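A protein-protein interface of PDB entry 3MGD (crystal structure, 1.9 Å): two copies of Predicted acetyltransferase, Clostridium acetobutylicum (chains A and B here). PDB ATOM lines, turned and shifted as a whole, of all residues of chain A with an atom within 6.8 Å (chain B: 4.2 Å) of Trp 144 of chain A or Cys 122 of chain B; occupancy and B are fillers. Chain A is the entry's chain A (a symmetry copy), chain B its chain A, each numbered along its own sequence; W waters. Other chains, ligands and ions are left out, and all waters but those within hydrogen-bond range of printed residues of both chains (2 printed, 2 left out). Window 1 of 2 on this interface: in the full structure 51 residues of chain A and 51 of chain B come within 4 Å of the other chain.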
ATOM      1  N   PHE A  73      30.926 -11.073  20.573  1.00  0.00           N
ATOM      2  CA  PHE A  73      31.923 -11.034  19.516  1.00  0.00           C
ATOM      3  C   PHE A  73      33.031 -10.082  19.978  1.00  0.00           C
ATOM      4  O   PHE A  73      32.847  -9.346  20.942  1.00  0.00           O
ATOM      5  CB  PHE A  73      31.295 -10.528  18.212  1.00  0.00           C
ATOM      6  CG  PHE A  73      30.196 -11.412  17.675  1.00  0.00           C
ATOM      7  CD1 PHE A  73      30.489 -12.486  16.842  1.00  0.00           C
ATOM      8  CD2 PHE A  73      28.869 -11.166  17.999  1.00  0.00           C
ATOM      9  CE1 PHE A  73      29.479 -13.304  16.338  1.00  0.00           C
ATOM     10  CE2 PHE A  73      27.856 -11.981  17.510  1.00  0.00           C
ATOM     11  CZ  PHE A  73      28.162 -13.048  16.674  1.00  0.00           C
ATOM     12  N   LYS A  84      26.041  -8.701  20.637  1.00  0.00           N
ATOM     13  CA  LYS A  84      24.953  -8.573  19.683  1.00  0.00           C
ATOM     14  C   LYS A  84      23.764  -9.374  20.167  1.00  0.00           C
ATOM     15  O   LYS A  84      23.922 -10.343  20.907  1.00  0.00           O
ATOM     16  CB  LYS A  84      25.373  -9.090  18.300  1.00  0.00           C
ATOM     17  CG  LYS A  84      26.324  -8.141  17.533  1.00  0.00           C
ATOM     18  CD  LYS A  84      26.600  -8.659  16.121  1.00  0.00           C
ATOM     19  CE  LYS A  84      27.364  -7.644  15.276  1.00  0.00           C
ATOM     20  NZ  LYS A  84      27.644  -8.184  13.917  1.00  0.00           N
ATOM     21  N   CYS A 122      21.246  -9.221  14.910  1.00  0.00           N
ATOM     22  CA  CYS A 122      21.446  -9.943  13.669  1.00  0.00           C
ATOM     23  C   CYS A 122      20.558 -11.158  13.685  1.00  0.00           C
ATOM     24  O   CYS A 122      20.015 -11.513  14.726  1.00  0.00           O
ATOM     25  CB  CYS A 122      22.921 -10.326  13.506  1.00  0.00           C
ATOM     26  SG  CYS A 122      23.585 -11.352  14.838  1.00  0.00           S
ATOM     27  N   THR A 141      23.816  -8.384   4.285  1.00  0.00           N
ATOM     28  CA  THR A 141      25.186  -8.462   4.801  1.00  0.00           C
ATOM     29  C   THR A 141      26.068  -9.399   3.972  1.00  0.00           C
ATOM     30  O   THR A 141      26.304 -10.546   4.363  1.00  0.00           O
ATOM     31  CB  THR A 141      25.227  -8.972   6.262  1.00  0.00           C
ATOM     32  OG1 THR A 141      24.307  -8.231   7.073  1.00  0.00           O
ATOM     33  CG2 THR A 141      26.638  -8.828   6.836  1.00  0.00           C
ATOM     34  N   ASP A 142      26.565  -8.907   2.840  1.00  0.00           N
ATOM     35  CA  ASP A 142      27.410  -9.712   1.959  1.00  0.00           C
ATOM     36  C   ASP A 142      28.707 -10.198   2.624  1.00  0.00           C
ATOM     37  O   ASP A 142      29.414 -11.042   2.070  1.00  0.00           O
ATOM     38  CB  ASP A 142      27.738  -8.936   0.677  1.00  0.00           C
ATOM     39  CG  ASP A 142      26.518  -8.722  -0.208  1.00  0.00           C
ATOM     40  OD1 ASP A 142      25.492  -9.405   0.007  1.00  0.00           O
ATOM     41  OD2 ASP A 142      26.585  -7.877  -1.127  1.00  0.00           O
ATOM     42  N   GLU A 143      29.018  -9.673   3.808  1.00  0.00           N
ATOM     43  CA  GLU A 143      30.259 -10.016   4.480  1.00  0.00           C
ATOM     44  C   GLU A 143      30.263 -11.362   5.221  1.00  0.00           C
ATOM     45  O   GLU A 143      31.324 -11.889   5.482  1.00  0.00           O
ATOM     46  CB  GLU A 143      30.691  -8.903   5.443  1.00  0.00           C
ATOM     47  CG  GLU A 143      31.215  -7.646   4.763  1.00  0.00           C
ATOM     48  CD  GLU A 143      30.103  -6.692   4.373  1.00  0.00           C
ATOM     49  OE1 GLU A 143      28.992  -6.803   4.945  1.00  0.00           O
ATOM     50  OE2 GLU A 143      30.343  -5.829   3.500  1.00  0.00           O
ATOM     51  N   TRP A 144      29.097 -11.898   5.576  1.00  0.00           N
ATOM     52  CA  TRP A 144      29.039 -13.153   6.345  1.00  0.00           C
ATOM     53  C   TRP A 144      29.243 -14.362   5.458  1.00  0.00           C
ATOM     54  O   TRP A 144      28.487 -14.555   4.509  1.00  0.00           O
ATOM     55  CB  TRP A 144      27.685 -13.329   7.019  1.00  0.00           C
ATOM     56  CG  TRP A 144      27.580 -12.717   8.350  1.00  0.00           C
ATOM     57  CD1 TRP A 144      27.097 -11.483   8.636  1.00  0.00           C
ATOM     58  CD2 TRP A 144      27.959 -13.305   9.602  1.00  0.00           C
ATOM     59  NE1 TRP A 144      27.146 -11.259   9.989  1.00  0.00           N
ATOM     60  CE2 TRP A 144      27.677 -12.362  10.604  1.00  0.00           C
ATOM     61  CE3 TRP A 144      28.510 -14.533   9.972  1.00  0.00           C
ATOM     62  CZ2 TRP A 144      27.920 -12.611  11.951  1.00  0.00           C
ATOM     63  CZ3 TRP A 144      28.747 -14.777  11.310  1.00  0.00           C
ATOM     64  CH2 TRP A 144      28.459 -13.822  12.279  1.00  0.00           C
ATOM     65  N   LEU A 145      30.224 -15.197   5.795  1.00  0.00           N
ATOM     66  CA  LEU A 145      30.515 -16.393   5.004  1.00  0.00           C
ATOM     67  C   LEU A 145      30.580 -17.600   5.922  1.00  0.00           C
ATOM     68  O   LEU A 145      30.935 -17.472   7.092  1.00  0.00           O
ATOM     69  CB  LEU A 145      31.847 -16.235   4.252  1.00  0.00           C
ATOM     70  CG  LEU A 145      32.015 -14.991   3.377  1.00  0.00           C
ATOM     71  CD1 LEU A 145      33.428 -14.914   2.776  1.00  0.00           C
ATOM     72  CD2 LEU A 145      30.965 -14.929   2.278  1.00  0.00           C
ATOM     73  N   GLU A 146      30.253 -18.775   5.398  1.00  0.00           N
ATOM     74  CA  GLU A 146      30.228 -19.967   6.227  1.00  0.00           C
ATOM     75  C   GLU A 146      30.924 -21.161   5.584  1.00  0.00           C
ATOM     76  O   GLU A 146      30.808 -21.391   4.385  1.00  0.00           O
ATOM     77  CB  GLU A 146      28.784 -20.326   6.585  1.00  0.00           C
ATOM     78  CG  GLU A 146      27.965 -19.123   7.043  1.00  0.00           C
ATOM     79  CD  GLU A 146      26.639 -19.519   7.666  1.00  0.00           C
ATOM     80  OE1 GLU A 146      26.114 -20.602   7.318  1.00  0.00           O
ATOM     81  OE2 GLU A 146      26.125 -18.746   8.508  1.00  0.00           O
ATOM     82  N   LEU A 147      31.644 -21.914   6.407  1.00  0.00           N
ATOM     83  CA  LEU A 147      32.360 -23.108   5.967  1.00  0.00           C
ATOM     84  C   LEU A 147      31.742 -24.319   6.644  1.00  0.00           C
ATOM     85  O   LEU A 147      31.581 -24.346   7.865  1.00  0.00           O
ATOM     86  CB  LEU A 147      33.842 -23.018   6.352  1.00  0.00           C
ATOM     87  CG  LEU A 147      34.737 -24.197   5.953  1.00  0.00           C
ATOM     88  CD1 LEU A 147      34.886 -24.234   4.448  1.00  0.00           C
ATOM     89  CD2 LEU A 147      36.120 -24.115   6.630  1.00  0.00           C
ATOM     90  N   GLY B  85      32.033 -22.316  15.116  1.00  0.00           N
ATOM     91  CA  GLY B  85      33.297 -21.642  15.353  1.00  0.00           C
ATOM     92  C   GLY B  85      33.213 -20.343  14.578  1.00  0.00           C
ATOM     93  O   GLY B  85      32.802 -20.332  13.424  1.00  0.00           O
ATOM     94  N   TYR B  86      33.584 -19.245  15.219  1.00  0.00           N
ATOM     95  CA  TYR B  86      33.523 -17.930  14.593  1.00  0.00           C
ATOM     96  C   TYR B  86      34.960 -17.452  14.415  1.00  0.00           C
ATOM     97  O   TYR B  86      35.672 -17.223  15.392  1.00  0.00           O
ATOM     98  CB  TYR B  86      32.753 -16.951  15.491  1.00  0.00           C
ATOM     99  CG  TYR B  86      32.742 -15.525  14.974  1.00  0.00           C
ATOM    100  CD1 TYR B  86      31.922 -15.156  13.916  1.00  0.00           C
ATOM    101  CD2 TYR B  86      33.553 -14.551  15.548  1.00  0.00           C
ATOM    102  CE1 TYR B  86      31.913 -13.847  13.435  1.00  0.00           C
ATOM    103  CE2 TYR B  86      33.553 -13.243  15.077  1.00  0.00           C
ATOM    104  CZ  TYR B  86      32.730 -12.900  14.030  1.00  0.00           C
ATOM    105  OH  TYR B  86      32.737 -11.604  13.567  1.00  0.00           O
ATOM    106  N   ILE B  87      35.392 -17.318  13.169  1.00  0.00           N
ATOM    107  CA  ILE B  87      36.779 -16.953  12.907  1.00  0.00           C
ATOM    108  C   ILE B  87      36.953 -15.441  12.877  1.00  0.00           C
ATOM    109  O   ILE B  87      36.108 -14.714  12.347  1.00  0.00           O
ATOM    110  CB  ILE B  87      37.292 -17.643  11.617  1.00  0.00           C
ATOM    111  CG1 ILE B  87      37.452 -19.154  11.913  1.00  0.00           C
ATOM    112  CG2 ILE B  87      38.564 -16.968  11.094  1.00  0.00           C
ATOM    113  CD1 ILE B  87      38.095 -19.958  10.808  1.00  0.00           C
ATOM    114  N   ILE B 121      31.646 -23.420  10.561  1.00  0.00           N
ATOM    115  CA  ILE B 121      32.452 -22.238  10.870  1.00  0.00           C
ATOM    116  C   ILE B 121      31.875 -21.042  10.138  1.00  0.00           C
ATOM    117  O   ILE B 121      31.335 -21.175   9.048  1.00  0.00           O
ATOM    118  CB  ILE B 121      33.903 -22.419  10.419  1.00  0.00           C
ATOM    119  CG1 ILE B 121      34.399 -23.818  10.780  1.00  0.00           C
ATOM    120  CG2 ILE B 121      34.790 -21.354  11.046  1.00  0.00           C
ATOM    121  CD1 ILE B 121      34.308 -24.120  12.245  1.00  0.00           C
ATOM    122  N   CYS B 122      31.961 -19.868  10.740  1.00  0.00           N
ATOM    123  CA  CYS B 122      31.469 -18.687  10.058  1.00  0.00           C
ATOM    124  C   CYS B 122      32.405 -17.547  10.358  1.00  0.00           C
ATOM    125  O   CYS B 122      33.241 -17.653  11.249  1.00  0.00           O
ATOM    126  CB  CYS B 122      30.037 -18.371  10.504  1.00  0.00           C
ATOM    127  SG  CYS B 122      29.845 -18.087  12.278  1.00  0.00           S
ATOM    128  N   LEU B 123      32.287 -16.471   9.594  1.00  0.00           N
ATOM    129  CA  LEU B 123      33.127 -15.293   9.798  1.00  0.00           C
ATOM    130  C   LEU B 123      32.529 -14.121   9.047  1.00  0.00           C
ATOM    131  O   LEU B 123      31.637 -14.301   8.212  1.00  0.00           O
ATOM    132  CB  LEU B 123      34.555 -15.553   9.306  1.00  0.00           C
ATOM    133  CG  LEU B 123      34.763 -16.002   7.854  1.00  0.00           C
ATOM    134  CD1 LEU B 123      34.530 -14.878   6.849  1.00  0.00           C
ATOM    135  CD2 LEU B 123      36.154 -16.571   7.676  1.00  0.00           C
ATOM    136  N   VAL B 124      33.022 -12.924   9.349  1.00  0.00           N
ATOM    137  CA  VAL B 124      32.702 -11.739   8.569  1.00  0.00           C
ATOM    138  C   VAL B 124      33.933 -11.339   7.754  1.00  0.00           C
ATOM    139  O   VAL B 124      34.994 -11.039   8.304  1.00  0.00           O
ATOM    140  CB  VAL B 124      32.280 -10.562   9.469  1.00  0.00           C
ATOM    141  CG1 VAL B 124      32.075  -9.303   8.636  1.00  0.00           C
ATOM    142  CG2 VAL B 124      31.004 -10.916  10.272  1.00  0.00           C
ATOM    143  N   THR B 141      26.453 -16.093   2.044  1.00  0.00           N
ATOM    144  CA  THR B 141      25.292 -16.343   2.904  1.00  0.00           C
ATOM    145  C   THR B 141      24.277 -15.198   2.860  1.00  0.00           C
ATOM    146  O   THR B 141      24.239 -14.360   3.767  1.00  0.00           O
ATOM    147  CB  THR B 141      25.699 -16.536   4.385  1.00  0.00           C
ATOM    148  OG1 THR B 141      26.758 -17.494   4.489  1.00  0.00           O
ATOM    149  CG2 THR B 141      24.500 -17.013   5.207  1.00  0.00           C
ATOM    150  N   TRP B 144      21.998 -13.874   6.184  1.00  0.00           N
ATOM    151  CA  TRP B 144      22.354 -13.089   7.377  1.00  0.00           C
ATOM    152  C   TRP B 144      21.991 -11.629   7.213  1.00  0.00           C
ATOM    153  O   TRP B 144      22.460 -10.986   6.277  1.00  0.00           O
ATOM    154  CB  TRP B 144      23.852 -13.138   7.648  1.00  0.00           C
ATOM    155  CG  TRP B 144      24.286 -14.266   8.481  1.00  0.00           C
ATOM    156  CD1 TRP B 144      24.746 -15.464   8.043  1.00  0.00           C
ATOM    157  CD2 TRP B 144      24.315 -14.320   9.913  1.00  0.00           C
ATOM    158  NE1 TRP B 144      25.065 -16.266   9.110  1.00  0.00           N
ATOM    159  CE2 TRP B 144      24.804 -15.587  10.271  1.00  0.00           C
ATOM    160  CE3 TRP B 144      23.974 -13.422  10.927  1.00  0.00           C
ATOM    161  CZ2 TRP B 144      24.967 -15.976  11.597  1.00  0.00           C
ATOM    162  CZ3 TRP B 144      24.141 -13.810  12.241  1.00  0.00           C
ATOM    163  CH2 TRP B 144      24.625 -15.073  12.563  1.00  0.00           C
ATOM    164  N   GLU B 146      21.304  -7.722   9.397  1.00  0.00           N
ATOM    165  CA  GLU B 146      21.641  -7.021  10.623  1.00  0.00           C
ATOM    166  C   GLU B 146      20.874  -5.715  10.800  1.00  0.00           C
ATOM    167  O   GLU B 146      20.663  -4.972   9.847  1.00  0.00           O
ATOM    168  CB  GLU B 146      23.149  -6.762  10.680  1.00  0.00           C
ATOM    169  CG  GLU B 146      23.980  -7.984  10.307  1.00  0.00           C
ATOM    170  CD  GLU B 146      25.451  -7.817  10.640  1.00  0.00           C
ATOM    171  OE1 GLU B 146      25.928  -6.658  10.675  1.00  0.00           O
ATOM    172  OE2 GLU B 146      26.129  -8.846  10.870  1.00  0.00           O
HETATM  173  O   HOH W   1      22.960 -10.779   3.384  1.00  0.00           O
HETATM  174  O   HOH W   2      27.180 -13.494   2.094  1.00  0.00           O
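The backbone NH of Leu 147 of chain A sits at hydrogen-bond distance from the backbone carbonyl oxygen of Ile 121 of chain B. The backbone carbonyl oxygen (O) of Leu 123 of chain B lies within hydrogen-bond range of the backbone NH (N) of Leu 145 of chain A (2.9 Å). OG1 of Thr 141 of chain B is in hydrogen-bond range of O of Trp 144 of chain A, at 3.4 Å. OG1 of Thr 141 of chain A lies within hydrogen-bond range of O of Trp 144 of chain B, 3.4 Å away. The indole nitrogen of Trp 144 of chain B sits at hydrogen-bond distance from the side-chain carboxylate of Glu 146 of chain A (2.8 Å). The side-chain amino group (NZ) of Lys 84 of chain A is in salt-bridge range of the side-chain carboxylate (OE2) of Glu 146 of chain B. OE2 of Glu 146 of chain B sits at hydrogen-bond distance from NE1 of Trp 144 of chain A (2.8 Å).
The backbone carbonyl oxygen of Gly 85 of chain B lies within hydrogen-bond range of the backbone NH of Cys 122 of chain B, 2.9 Å away. The backbone NH of Ile 87 of chain B sits at hydrogen-bond distance from the backbone carbonyl oxygen of Cys 122 of chain B.
Phe 73 of chain A touches Tyr 86 of chain B. Trp 144 of chain B touches Cys 122 of chain A (CZ3 to SG, 3.6 Å). OG1 of Thr 141 of chain A touches CG of Glu 146 of chain B (3.3 Å). CA of Val 124 of chain B touches O of Glu 143 of chain A (3.4 Å). CZ3 of Trp 144 of chain A touches SG of Cys 122 of chain B (3.6 Å). Val 124 of chain B touches Trp 144 of chain A. CG of Trp 144 of chain B touches CG of Trp 144 of chain A (3.6 Å). Leu 145 of chain A touches Thr 141 of chain B. O of Ile 121 of chain B touches CA of Glu 146 of chain A (3.3 Å). OG1 of Thr 141 of chain B touches CG of Glu 146 of chain A, at 3.3 Å.
Printed residues of chain B within 4 Å of Cys 122 of chain A: Trp 144 (3.6 Å). Asp 142 of chain A touches none of the printed residues of chain B. Printed residues of chain B within 4 Å of Leu 145 of chain A: Cys 122 (3.2 Å), Leu 123 (2.9 Å) and Thr 141 (3.9 Å). Ile 87 of chain B touches none of the printed residues of chain A. Printed residues of chain A within 4 Å of Ile 121 of chain B: Glu 146 and Leu 147. Cys 122 of chain B touches just these residues of chain A: Trp 144 (3.6 Å) and Leu 145 (3.2 Å). Of the printed residues of chain A, Glu 146 of chain B touches Lys 84, Thr 141 and Trp 144. The nearest printed residue of chain B that does not touch Phe 73 of chain A is Trp 144 of chain B (5.8 Å).
Along chain B the printed residues that touch a printed residue of chain A span positions 86 to 146. Printed residues of chain A that touch a printed residue of chain B: Phe 73, Lys 84, Cys 122, Thr 141, Glu 143, Trp 144, Leu 145, Glu 146 and Leu 147. Hydrophobic or aromatic side chains of chain A that line the printed part of chain B: Phe 73, Trp 144 and Leu 145. Among the printed residues, 21 pairs touch across the chains. Among the printed residues, Asp or Glu carboxylates within 4 Å of a Lys or Arg side-chain nitrogen of the other chain: Lys 84 of chain A with Glu 146 of chain B.
Cys 122 of chain A touches Trp 144 of chain B, and with the chains exchanged Trp 144 of chain A touches Cys 122 of chain B. Thr 141 of chain A touches Trp 144 of chain B, and with the chains exchanged Trp 144 of chain A touches Thr 141 of chain B. Thr 141 of chain A touches Glu 146 of chain B, and with the chains exchanged Glu 146 of chain A touches Thr 141 of chain B. Trp 144 of chain A touches Glu 146 of chain B, and with the chains exchanged Glu 146 of chain A touches Trp 144 of chain B.
Water W1 lies within hydrogen-bond range of the backbone NH (N) of Thr 141 of chain A and the backbone carbonyl oxygen (O) of Trp 144 of chain B. Water W2 lies within hydrogen-bond range of the backbone NH (N) of Thr 141 of chain B, the backbone carbonyl oxygen (O) of Trp 144 of chain A and the backbone carbonyl oxygen (O) of Asp 142 of chain A.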
